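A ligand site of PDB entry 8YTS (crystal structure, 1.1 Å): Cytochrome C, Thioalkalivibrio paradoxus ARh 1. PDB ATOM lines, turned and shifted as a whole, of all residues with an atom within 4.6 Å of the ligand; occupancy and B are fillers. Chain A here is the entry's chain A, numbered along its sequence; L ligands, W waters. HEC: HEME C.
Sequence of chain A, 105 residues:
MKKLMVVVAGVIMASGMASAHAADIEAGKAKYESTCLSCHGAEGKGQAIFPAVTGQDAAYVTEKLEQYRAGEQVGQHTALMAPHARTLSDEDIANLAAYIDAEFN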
ATOM      1  N   THR A  35      11.279  -4.851 -19.187  1.00  0.00           N
ATOM      2  CA  THR A  35      10.593  -5.579 -20.259  1.00  0.00           C
ATOM      3  C   THR A  35       9.200  -5.019 -20.593  1.00  0.00           C
ATOM      4  O   THR A  35       8.637  -5.382 -21.632  1.00  0.00           O
ATOM      5  CB  THR A  35      10.444  -7.035 -19.742  1.00  0.00           C
ATOM      6  OG1 THR A  35      11.740  -7.531 -19.369  1.00  0.00           O
ATOM      7  CG2 THR A  35       9.847  -7.994 -20.726  1.00  0.00           C
ATOM      8  N   CYS A  36       8.607  -4.205 -19.725  1.00  0.00           N
ATOM      9  CA  CYS A  36       7.200  -3.839 -19.839  1.00  0.00           C
ATOM     10  C   CYS A  36       6.997  -2.327 -19.850  1.00  0.00           C
ATOM     11  O   CYS A  36       6.086  -1.814 -20.498  1.00  0.00           O
ATOM     12  CB  CYS A  36       6.372  -4.450 -18.707  1.00  0.00           C
ATOM     13  SG  CYS A  36       6.740  -6.112 -18.266  1.00  0.00           S
ATOM     14  N   SER A  38       8.495   0.268 -21.002  1.00  0.00           N
ATOM     15  CA  SER A  38       8.603   1.041 -22.247  1.00  0.00           C
ATOM     16  C   SER A  38       7.238   1.273 -22.900  1.00  0.00           C
ATOM     17  O   SER A  38       6.972   2.331 -23.455  1.00  0.00           O
ATOM     18  CB  SER A  38       9.579   0.424 -23.174  1.00  0.00           C
ATOM     19  OG  SER A  38       9.137  -0.847 -23.574  1.00  0.00           O
ATOM     20  N   CYS A  39       6.360   0.239 -22.842  1.00  0.00           N
ATOM     21  CA  CYS A  39       5.013   0.371 -23.386  1.00  0.00           C
ATOM     22  C   CYS A  39       3.968   0.778 -22.348  1.00  0.00           C
ATOM     23  O   CYS A  39       3.147   1.629 -22.621  1.00  0.00           O
ATOM     24  CB  CYS A  39       4.560  -0.931 -24.016  1.00  0.00           C
ATOM     25  SG  CYS A  39       5.534  -1.335 -25.498  1.00  0.00           S
ATOM     26  N   HIS A  40       3.972   0.127 -21.182  1.00  0.00           N
ATOM     27  CA  HIS A  40       2.890   0.342 -20.235  1.00  0.00           C
ATOM     28  C   HIS A  40       3.144   1.493 -19.256  1.00  0.00           C
ATOM     29  O   HIS A  40       2.187   1.896 -18.582  1.00  0.00           O
ATOM     30  CB  HIS A  40       2.520  -0.971 -19.530  1.00  0.00           C
ATOM     31  CG  HIS A  40       1.885  -1.957 -20.427  1.00  0.00           C
ATOM     32  ND1 HIS A  40       0.604  -1.814 -20.904  1.00  0.00           N
ATOM     33  CD2 HIS A  40       2.330  -3.135 -20.881  1.00  0.00           C
ATOM     34  CE1 HIS A  40       0.305  -2.903 -21.631  1.00  0.00           C
ATOM     35  NE2 HIS A  40       1.375  -3.755 -21.633  1.00  0.00           N
ATOM     36  N   PHE A  50      -1.142   2.406 -25.675  1.00  0.00           N
ATOM     37  CA  PHE A  50      -1.079   1.049 -25.149  1.00  0.00           C
ATOM     38  C   PHE A  50      -2.017   0.987 -23.950  1.00  0.00           C
ATOM     39  O   PHE A  50      -2.184   2.004 -23.271  1.00  0.00           O
ATOM     40  CB  PHE A  50       0.346   0.690 -24.718  1.00  0.00           C
ATOM     41  CG  PHE A  50       1.325   0.698 -25.856  1.00  0.00           C
ATOM     42  CD1 PHE A  50       1.165  -0.158 -26.908  1.00  0.00           C
ATOM     43  CD2 PHE A  50       2.430   1.528 -25.859  1.00  0.00           C
ATOM     44  CE1 PHE A  50       2.056  -0.190 -27.945  1.00  0.00           C
ATOM     45  CE2 PHE A  50       3.339   1.483 -26.901  1.00  0.00           C
ATOM     46  CZ  PHE A  50       3.151   0.611 -27.936  1.00  0.00           C
ATOM     47  N   PRO A  51      -2.598  -0.182 -23.585  1.00  0.00           N
ATOM     48  CA  PRO A  51      -3.499  -0.223 -22.466  1.00  0.00           C
ATOM     49  C   PRO A  51      -2.795   0.157 -21.174  1.00  0.00           C
ATOM     50  O   PRO A  51      -1.652  -0.217 -20.930  1.00  0.00           O
ATOM     51  CB  PRO A  51      -3.985  -1.680 -22.394  1.00  0.00           C
ATOM     52  CG  PRO A  51      -3.507  -2.359 -23.582  1.00  0.00           C
ATOM     53  CD  PRO A  51      -2.532  -1.468 -24.279  1.00  0.00           C
ATOM     54  N   ALA A  52      -3.510   0.851 -20.321  1.00  0.00           N
ATOM     55  CA  ALA A  52      -3.074   1.033 -18.963  1.00  0.00           C
ATOM     56  C   ALA A  52      -3.088  -0.316 -18.252  1.00  0.00           C
ATOM     57  O   ALA A  52      -3.907  -1.189 -18.549  1.00  0.00           O
ATOM     58  CB  ALA A  52      -3.957   2.013 -18.254  1.00  0.00           C
ATOM     59  N   VAL A  53      -2.220  -0.448 -17.259  1.00  0.00           N
ATOM     60  CA  VAL A  53      -2.260  -1.581 -16.348  1.00  0.00           C
ATOM     61  C   VAL A  53      -2.632  -1.117 -14.936  1.00  0.00           C
ATOM     62  O   VAL A  53      -2.372  -1.815 -13.989  1.00  0.00           O
ATOM     63  CB  VAL A  53      -0.973  -2.434 -16.408  1.00  0.00           C
ATOM     64  CG1 VAL A  53      -0.849  -3.180 -17.728  1.00  0.00           C
ATOM     65  CG2 VAL A  53       0.247  -1.603 -16.098  1.00  0.00           C
ATOM     66  N   GLN A  56      -6.084  -2.601 -11.660  1.00  0.00           N
ATOM     67  CA  GLN A  56      -6.352  -4.027 -11.819  1.00  0.00           C
ATOM     68  C   GLN A  56      -5.553  -4.785 -10.780  1.00  0.00           C
ATOM     69  O   GLN A  56      -4.411  -4.444 -10.434  1.00  0.00           O
ATOM     70  CB  GLN A  56      -6.072  -4.573 -13.234  1.00  0.00           C
ATOM     71  CG  GLN A  56      -4.830  -4.055 -13.950  1.00  0.00           C
ATOM     72  CD  GLN A  56      -4.734  -4.323 -15.453  1.00  0.00           C
ATOM     73  OE1 GLN A  56      -4.198  -5.320 -15.890  1.00  0.00           O
ATOM     74  NE2 GLN A  56      -5.154  -3.374 -16.276  1.00  0.00           N
ATOM     75  N   TYR A  60      -6.309 -10.455 -11.951  1.00  0.00           N
ATOM     76  CA  TYR A  60      -6.600 -10.034 -13.310  1.00  0.00           C
ATOM     77  C   TYR A  60      -5.341 -10.063 -14.185  1.00  0.00           C
ATOM     78  O   TYR A  60      -5.376 -10.542 -15.302  1.00  0.00           O
ATOM     79  CB  TYR A  60      -7.233  -8.645 -13.255  1.00  0.00           C
ATOM     80  CG  TYR A  60      -7.600  -8.141 -14.648  1.00  0.00           C
ATOM     81  CD1 TYR A  60      -6.685  -7.444 -15.416  1.00  0.00           C
ATOM     82  CD2 TYR A  60      -8.798  -8.493 -15.259  1.00  0.00           C
ATOM     83  CE1 TYR A  60      -6.977  -7.047 -16.716  1.00  0.00           C
ATOM     84  CE2 TYR A  60      -9.096  -8.113 -16.561  1.00  0.00           C
ATOM     85  CZ  TYR A  60      -8.192  -7.366 -17.291  1.00  0.00           C
ATOM     86  OH  TYR A  60      -8.493  -6.974 -18.572  1.00  0.00           O
ATOM     87  N   VAL A  61      -4.263  -9.481 -13.670  1.00  0.00           N
ATOM     88  CA  VAL A  61      -3.019  -9.417 -14.432  1.00  0.00           C
ATOM     89  C   VAL A  61      -2.506 -10.828 -14.713  1.00  0.00           C
ATOM     90  O   VAL A  61      -2.048 -11.124 -15.802  1.00  0.00           O
ATOM     91  CB  VAL A  61      -2.000  -8.544 -13.717  1.00  0.00           C
ATOM     92  CG1 VAL A  61      -0.650  -8.623 -14.407  1.00  0.00           C
ATOM     93  CG2 VAL A  61      -2.461  -7.107 -13.572  1.00  0.00           C
ATOM     94  N   LYS A  64      -4.540 -12.433 -17.490  1.00  0.00           N
ATOM     95  CA  LYS A  64      -4.210 -11.868 -18.804  1.00  0.00           C
ATOM     96  C   LYS A  64      -2.850 -12.358 -19.288  1.00  0.00           C
ATOM     97  O   LYS A  64      -2.702 -12.771 -20.456  1.00  0.00           O
ATOM     98  CB  LYS A  64      -4.243 -10.348 -18.787  1.00  0.00           C
ATOM     99  CG  LYS A  64      -5.643  -9.774 -18.738  1.00  0.00           C
ATOM    100  CD  LYS A  64      -6.299  -9.897 -20.150  1.00  0.00           C
ATOM    101  CE  LYS A  64      -7.783  -9.799 -20.215  1.00  0.00           C
ATOM    102  NZ  LYS A  64      -8.355 -10.967 -19.513  1.00  0.00           N
ATOM    103  N   LEU A  65      -1.826 -12.285 -18.438  1.00  0.00           N
ATOM    104  CA  LEU A  65      -0.499 -12.726 -18.864  1.00  0.00           C
ATOM    105  C   LEU A  65      -0.498 -14.205 -19.243  1.00  0.00           C
ATOM    106  O   LEU A  65       0.159 -14.603 -20.212  1.00  0.00           O
ATOM    107  CB  LEU A  65       0.570 -12.425 -17.825  1.00  0.00           C
ATOM    108  CG  LEU A  65       0.847 -10.958 -17.616  1.00  0.00           C
ATOM    109  CD1 LEU A  65       1.810 -10.787 -16.436  1.00  0.00           C
ATOM    110  CD2 LEU A  65       1.416 -10.346 -18.875  1.00  0.00           C
ATOM    111  N   TYR A  68      -1.981 -14.454 -22.784  1.00  0.00           N
ATOM    112  CA  TYR A  68      -1.009 -14.069 -23.823  1.00  0.00           C
ATOM    113  C   TYR A  68       0.069 -15.131 -23.972  1.00  0.00           C
ATOM    114  O   TYR A  68       0.420 -15.487 -25.114  1.00  0.00           O
ATOM    115  CB  TYR A  68      -0.399 -12.708 -23.526  1.00  0.00           C
ATOM    116  CG  TYR A  68      -1.333 -11.541 -23.730  1.00  0.00           C
ATOM    117  CD1 TYR A  68      -1.790 -11.205 -24.994  1.00  0.00           C
ATOM    118  CD2 TYR A  68      -1.785 -10.786 -22.657  1.00  0.00           C
ATOM    119  CE1 TYR A  68      -2.662 -10.133 -25.179  1.00  0.00           C
ATOM    120  CE2 TYR A  68      -2.684  -9.748 -22.837  1.00  0.00           C
ATOM    121  CZ  TYR A  68      -3.145  -9.423 -24.086  1.00  0.00           C
ATOM    122  OH  TYR A  68      -4.020  -8.386 -24.180  1.00  0.00           O
ATOM    123  N   VAL A  74      -6.374 -12.426 -27.626  1.00  0.00           N
ATOM    124  CA  VAL A  74      -7.040 -11.632 -26.609  1.00  0.00           C
ATOM    125  C   VAL A  74      -7.711 -10.511 -27.401  1.00  0.00           C
ATOM    126  O   VAL A  74      -8.769 -10.731 -27.996  1.00  0.00           O
ATOM    127  CB  VAL A  74      -6.090 -11.253 -25.473  1.00  0.00           C
ATOM    128  CG1 VAL A  74      -6.792 -10.480 -24.377  1.00  0.00           C
ATOM    129  CG2 VAL A  74      -5.393 -12.471 -24.900  1.00  0.00           C
ATOM    130  N   GLY A  75      -7.052  -9.389 -27.556  1.00  0.00           N
ATOM    131  CA  GLY A  75      -7.614  -8.301 -28.317  1.00  0.00           C
ATOM    132  C   GLY A  75      -7.036  -8.197 -29.718  1.00  0.00           C
ATOM    133  O   GLY A  75      -6.200  -8.979 -30.156  1.00  0.00           O
ATOM    134  N   GLN A  76      -7.458  -7.123 -30.384  1.00  0.00           N
ATOM    135  CA  GLN A  76      -7.076  -6.898 -31.766  1.00  0.00           C
ATOM    136  C   GLN A  76      -5.571  -6.781 -31.968  1.00  0.00           C
ATOM    137  O   GLN A  76      -5.095  -7.026 -33.076  1.00  0.00           O
ATOM    138  CB  GLN A  76      -7.754  -5.598 -32.198  1.00  0.00           C
ATOM    139  CG  GLN A  76      -7.510  -5.156 -33.612  1.00  0.00           C
ATOM    140  CD  GLN A  76      -8.046  -6.129 -34.618  1.00  0.00           C
ATOM    141  OE1 GLN A  76      -9.049  -6.801 -34.427  1.00  0.00           O
ATOM    142  NE2 GLN A  76      -7.380  -6.150 -35.764  1.00  0.00           N
ATOM    143  N   HIS A  77      -4.845  -6.347 -30.945  1.00  0.00           N
ATOM    144  CA  HIS A  77      -3.411  -6.124 -31.025  1.00  0.00           C
ATOM    145  C   HIS A  77      -2.607  -7.134 -30.236  1.00  0.00           C
ATOM    146  O   HIS A  77      -1.496  -6.860 -29.794  1.00  0.00           O
ATOM    147  CB  HIS A  77      -3.076  -4.701 -30.570  1.00  0.00           C
ATOM    148  CG  HIS A  77      -3.749  -3.699 -31.449  1.00  0.00           C
ATOM    149  ND1 HIS A  77      -3.656  -3.718 -32.837  1.00  0.00           N
ATOM    150  CD2 HIS A  77      -4.659  -2.741 -31.165  1.00  0.00           C
ATOM    151  CE1 HIS A  77      -4.437  -2.787 -33.340  1.00  0.00           C
ATOM    152  NE2 HIS A  77      -5.067  -2.159 -32.345  1.00  0.00           N
ATOM    153  N   THR A  78      -3.130  -8.350 -30.134  1.00  0.00           N
ATOM    154  CA  THR A  78      -2.445  -9.429 -29.436  1.00  0.00           C
ATOM    155  C   THR A  78      -1.021  -9.589 -29.932  1.00  0.00           C
ATOM    156  O   THR A  78      -0.123  -9.847 -29.129  1.00  0.00           O
ATOM    157  CB  THR A  78      -3.231 -10.745 -29.599  1.00  0.00           C
ATOM    158  OG1 THR A  78      -4.446 -10.689 -28.889  1.00  0.00           O
ATOM    159  CG2 THR A  78      -2.467 -11.943 -29.098  1.00  0.00           C
ATOM    160  N   LEU A  80       1.165  -7.498 -30.747  1.00  0.00           N
ATOM    161  CA  LEU A  80       2.101  -6.577 -30.122  1.00  0.00           C
ATOM    162  C   LEU A  80       2.503  -6.990 -28.711  1.00  0.00           C
ATOM    163  O   LEU A  80       3.556  -6.594 -28.225  1.00  0.00           O
ATOM    164  CB  LEU A  80       1.530  -5.163 -30.109  1.00  0.00           C
ATOM    165  CG  LEU A  80       1.141  -4.599 -31.471  1.00  0.00           C
ATOM    166  CD1 LEU A  80       0.629  -3.176 -31.311  1.00  0.00           C
ATOM    167  CD2 LEU A  80       2.316  -4.621 -32.457  1.00  0.00           C
ATOM    168  N   MET A  81       1.636  -7.716 -28.019  1.00  0.00           N
ATOM    169  CA  MET A  81       1.812  -8.045 -26.603  1.00  0.00           C
ATOM    170  C   MET A  81       2.328  -9.459 -26.420  1.00  0.00           C
ATOM    171  O   MET A  81       3.175  -9.717 -25.564  1.00  0.00           O
ATOM    172  CB  MET A  81       0.470  -7.825 -25.873  1.00  0.00           C
ATOM    173  CG  MET A  81       0.467  -8.293 -24.437  1.00  0.00           C
ATOM    174  SD  MET A  81       1.794  -7.627 -23.420  1.00  0.00           S
ATOM    175  CE  MET A  81       1.650  -8.860 -22.102  1.00  0.00           C
ATOM    176  N   HIS A  84       5.901 -10.628 -25.539  1.00  0.00           N
ATOM    177  CA  HIS A  84       6.377 -10.214 -24.230  1.00  0.00           C
ATOM    178  C   HIS A  84       5.886 -11.094 -23.105  1.00  0.00           C
ATOM    179  O   HIS A  84       6.349 -10.922 -21.974  1.00  0.00           O
ATOM    180  CB  HIS A  84       6.041  -8.732 -23.971  1.00  0.00           C
ATOM    181  CG  HIS A  84       6.565  -7.868 -25.060  1.00  0.00           C
ATOM    182  ND1 HIS A  84       7.914  -7.666 -25.210  1.00  0.00           N
ATOM    183  CD2 HIS A  84       5.965  -7.225 -26.083  1.00  0.00           C
ATOM    184  CE1 HIS A  84       8.120  -6.925 -26.292  1.00  0.00           C
ATOM    185  NE2 HIS A  84       6.949  -6.666 -26.841  1.00  0.00           N
ATOM    186  N   LEU A  88       7.532 -15.933 -20.250  1.00  0.00           N
ATOM    187  CA  LEU A  88       7.378 -15.734 -18.823  1.00  0.00           C
ATOM    188  C   LEU A  88       7.070 -17.062 -18.138  1.00  0.00           C
ATOM    189  O   LEU A  88       6.207 -17.822 -18.567  1.00  0.00           O
ATOM    190  CB  LEU A  88       6.207 -14.785 -18.569  1.00  0.00           C
ATOM    191  CG  LEU A  88       6.373 -13.365 -19.098  1.00  0.00           C
ATOM    192  CD1 LEU A  88       5.094 -12.562 -18.850  1.00  0.00           C
ATOM    193  CD2 LEU A  88       7.573 -12.665 -18.502  1.00  0.00           C
ATOM    194  N   LEU A  96       5.203 -10.135 -11.515  1.00  0.00           N
ATOM    195  CA  LEU A  96       4.720  -8.978 -12.264  1.00  0.00           C
ATOM    196  C   LEU A  96       3.326  -8.537 -11.777  1.00  0.00           C
ATOM    197  O   LEU A  96       3.081  -7.351 -11.619  1.00  0.00           O
ATOM    198  CB  LEU A  96       4.664  -9.327 -13.744  1.00  0.00           C
ATOM    199  CG  LEU A  96       6.012  -9.352 -14.457  1.00  0.00           C
ATOM    200  CD1 LEU A  96       5.909 -10.124 -15.729  1.00  0.00           C
ATOM    201  CD2 LEU A  96       6.550  -7.946 -14.690  1.00  0.00           C
ATOM    202  N   ILE A 100       2.416  -4.914 -10.206  1.00  0.00           N
ATOM    203  CA  ILE A 100       1.410  -4.069 -10.832  1.00  0.00           C
ATOM    204  C   ILE A 100       0.300  -3.733  -9.831  1.00  0.00           C
ATOM    205  O   ILE A 100      -0.120  -2.584  -9.742  1.00  0.00           O
ATOM    206  CB  ILE A 100       0.883  -4.722 -12.115  1.00  0.00           C
ATOM    207  CG1 ILE A 100       1.976  -4.616 -13.191  1.00  0.00           C
ATOM    208  CG2 ILE A 100      -0.441  -4.114 -12.562  1.00  0.00           C
ATOM    209  CD1 ILE A 100       1.767  -5.493 -14.382  1.00  0.00           C
HETATM  210 FE   HEC L   1       1.428  -5.545 -22.496  1.00  0.00          FE
HETATM  211  CHA HEC L   1      -1.941  -5.889 -23.034  1.00  0.00           C
HETATM  212  CHB HEC L   1       1.064  -6.566 -19.319  1.00  0.00           C
HETATM  213  CHC HEC L   1       4.771  -5.796 -22.250  1.00  0.00           C
HETATM  214  CHD HEC L   1       1.723  -3.825 -25.364  1.00  0.00           C
HETATM  215  NA  HEC L   1      -0.127  -6.136 -21.410  1.00  0.00           N
HETATM  216  C1A HEC L   1      -1.442  -6.177 -21.743  1.00  0.00           C
HETATM  217  C2A HEC L   1      -2.268  -6.598 -20.652  1.00  0.00           C
HETATM  218  C3A HEC L   1      -1.409  -6.737 -19.573  1.00  0.00           C
HETATM  219  C4A HEC L   1      -0.097  -6.449 -20.076  1.00  0.00           C
HETATM  220  CMA HEC L   1      -1.751  -7.158 -18.183  1.00  0.00           C
HETATM  221  CAA HEC L   1      -3.750  -6.720 -20.647  1.00  0.00           C
HETATM  222  CBA HEC L   1      -4.393  -5.344 -20.232  1.00  0.00           C
HETATM  223  CGA HEC L   1      -5.859  -5.456 -19.774  1.00  0.00           C
HETATM  224  O1A HEC L   1      -6.531  -6.367 -20.221  1.00  0.00           O
HETATM  225  O2A HEC L   1      -6.277  -4.654 -18.946  1.00  0.00           O
HETATM  226  NB  HEC L   1       2.712  -6.088 -21.032  1.00  0.00           N
HETATM  227  C1B HEC L   1       2.374  -6.487 -19.796  1.00  0.00           C
HETATM  228  C2B HEC L   1       3.536  -6.845 -19.040  1.00  0.00           C
HETATM  229  C3B HEC L   1       4.609  -6.727 -19.885  1.00  0.00           C
HETATM  230  C4B HEC L   1       4.035  -6.241 -21.139  1.00  0.00           C
HETATM  231  CMB HEC L   1       3.539  -7.294 -17.627  1.00  0.00           C
HETATM  232  CAB HEC L   1       6.049  -7.033 -19.646  1.00  0.00           C
HETATM  233  CBB HEC L   1       6.291  -8.517 -19.413  1.00  0.00           C
HETATM  234  NC  HEC L   1       2.953  -4.893 -23.581  1.00  0.00           N
HETATM  235  C1C HEC L   1       4.248  -5.084 -23.327  1.00  0.00           C
HETATM  236  C2C HEC L   1       5.098  -4.349 -24.256  1.00  0.00           C
HETATM  237  C3C HEC L   1       4.213  -3.711 -25.112  1.00  0.00           C
HETATM  238  C4C HEC L   1       2.884  -4.119 -24.688  1.00  0.00           C
HETATM  239  CMC HEC L   1       6.571  -4.291 -24.210  1.00  0.00           C
HETATM  240  CAC HEC L   1       4.527  -2.703 -26.168  1.00  0.00           C
HETATM  241  CBC HEC L   1       5.184  -3.265 -27.381  1.00  0.00           C
HETATM  242  ND  HEC L   1       0.140  -4.995 -23.956  1.00  0.00           N
HETATM  243  C1D HEC L   1       0.448  -4.320 -25.064  1.00  0.00           C
HETATM  244  C2D HEC L   1      -0.705  -4.194 -25.931  1.00  0.00           C
HETATM  245  C3D HEC L   1      -1.720  -4.829 -25.273  1.00  0.00           C
HETATM  246  C4D HEC L   1      -1.170  -5.278 -24.036  1.00  0.00           C
HETATM  247  CMD HEC L   1      -0.784  -3.549 -27.283  1.00  0.00           C
HETATM  248  CAD HEC L   1      -3.076  -5.142 -25.804  1.00  0.00           C
HETATM  249  CBD HEC L   1      -3.038  -6.430 -26.667  1.00  0.00           C
HETATM  250  CGD HEC L   1      -4.362  -6.864 -27.170  1.00  0.00           C
HETATM  251  O1D HEC L   1      -4.919  -7.862 -26.589  1.00  0.00           O
HETATM  252  O2D HEC L   1      -4.938  -6.224 -28.082  1.00  0.00           O
HETATM  253  O   HOH W   1      -6.394  -1.675 -19.137  1.00  0.00           O
HETATM  254  O   HOH W   2      -8.238  -3.664 -17.366  1.00  0.00           O
HETATM  255  O   HOH W   3      -7.140  -4.554 -27.898  1.00  0.00           O
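O of Thr 35 touches CMC of the ligand (3.5 Å). Phe 50 touches the ligand. Pro 51 touches the ligand. CD of Lys 64 touches O1A of the ligand (3.5 Å). Leu 65 touches the ligand. Val 74 touches the ligand. N of Gln 76 touches O2D of the ligand, at 3.5 Å. Leu 80 touches the ligand. His 84 touches the ligand (O to CBB, 3.5 Å). Hydrophobic or aromatic side chains that line the ligand: His 40, Phe 50, Pro 51, Tyr 60, Leu 65, Tyr 68, Val 74, His 77, Leu 80, Met 81 and His 84. Of the 26 residues printed, 19 come within 4 Å of the ligand.
Water W2 bridges O2A of the ligand and NE2 of Gln 56. Water W1 lies within hydrogen-bond range of O of Ala 52 (2.6 Å) and O2A of the ligand (3.0 Å).
A carbon (CAC) of the ligand is covalently linked to the side-chain sulfur (SG) of Cys 39. The backbone NH of His 77 sits at hydrogen-bond distance from an oxygen (O2D) of the ligand (2.9 Å). The side-chain amide nitrogen (NE2) of Gln 56 is in hydrogen-bond range of an oxygen (O2A) of the ligand. N of Thr 78 sits at hydrogen-bond distance from O2D of the ligand, at 3.5 Å. A ring nitrogen (NE2) of His 40 is bound to an iron atom (FE) of the ligand, 2.0 Å away. An oxygen (O1D) of the ligand sits at hydrogen-bond distance from the backbone NH (N) of Gly 75 (2.8 Å). The side-chain hydroxyl (OH) of Tyr 60 sits at hydrogen-bond distance from an oxygen (O1A) of the ligand, 2.6 Å away. O1D of the ligand lies within hydrogen-bond range of OH of Tyr 68, at 2.6 Å. The side-chain sulfur (SG) of Cys 36 is covalently linked to a carbon (CAB) of the ligand. SD of Met 81 binds FE of the ligand (2.3 Å).
The backbone carbonyl oxygen (O) of Ala 52 lies within hydrogen-bond range of the side-chain amide nitrogen (NE2) of Gln 56 (3.4 Å). The backbone NH of Val 74 is in hydrogen-bond range of the side-chain hydroxyl of Thr 78, 2.9 Å away. O of Pro 51 sits at hydrogen-bond distance from ND1 of His 40 (2.8 Å). O of Gly 75 sits at hydrogen-bond distance from OG1 of Thr 78.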
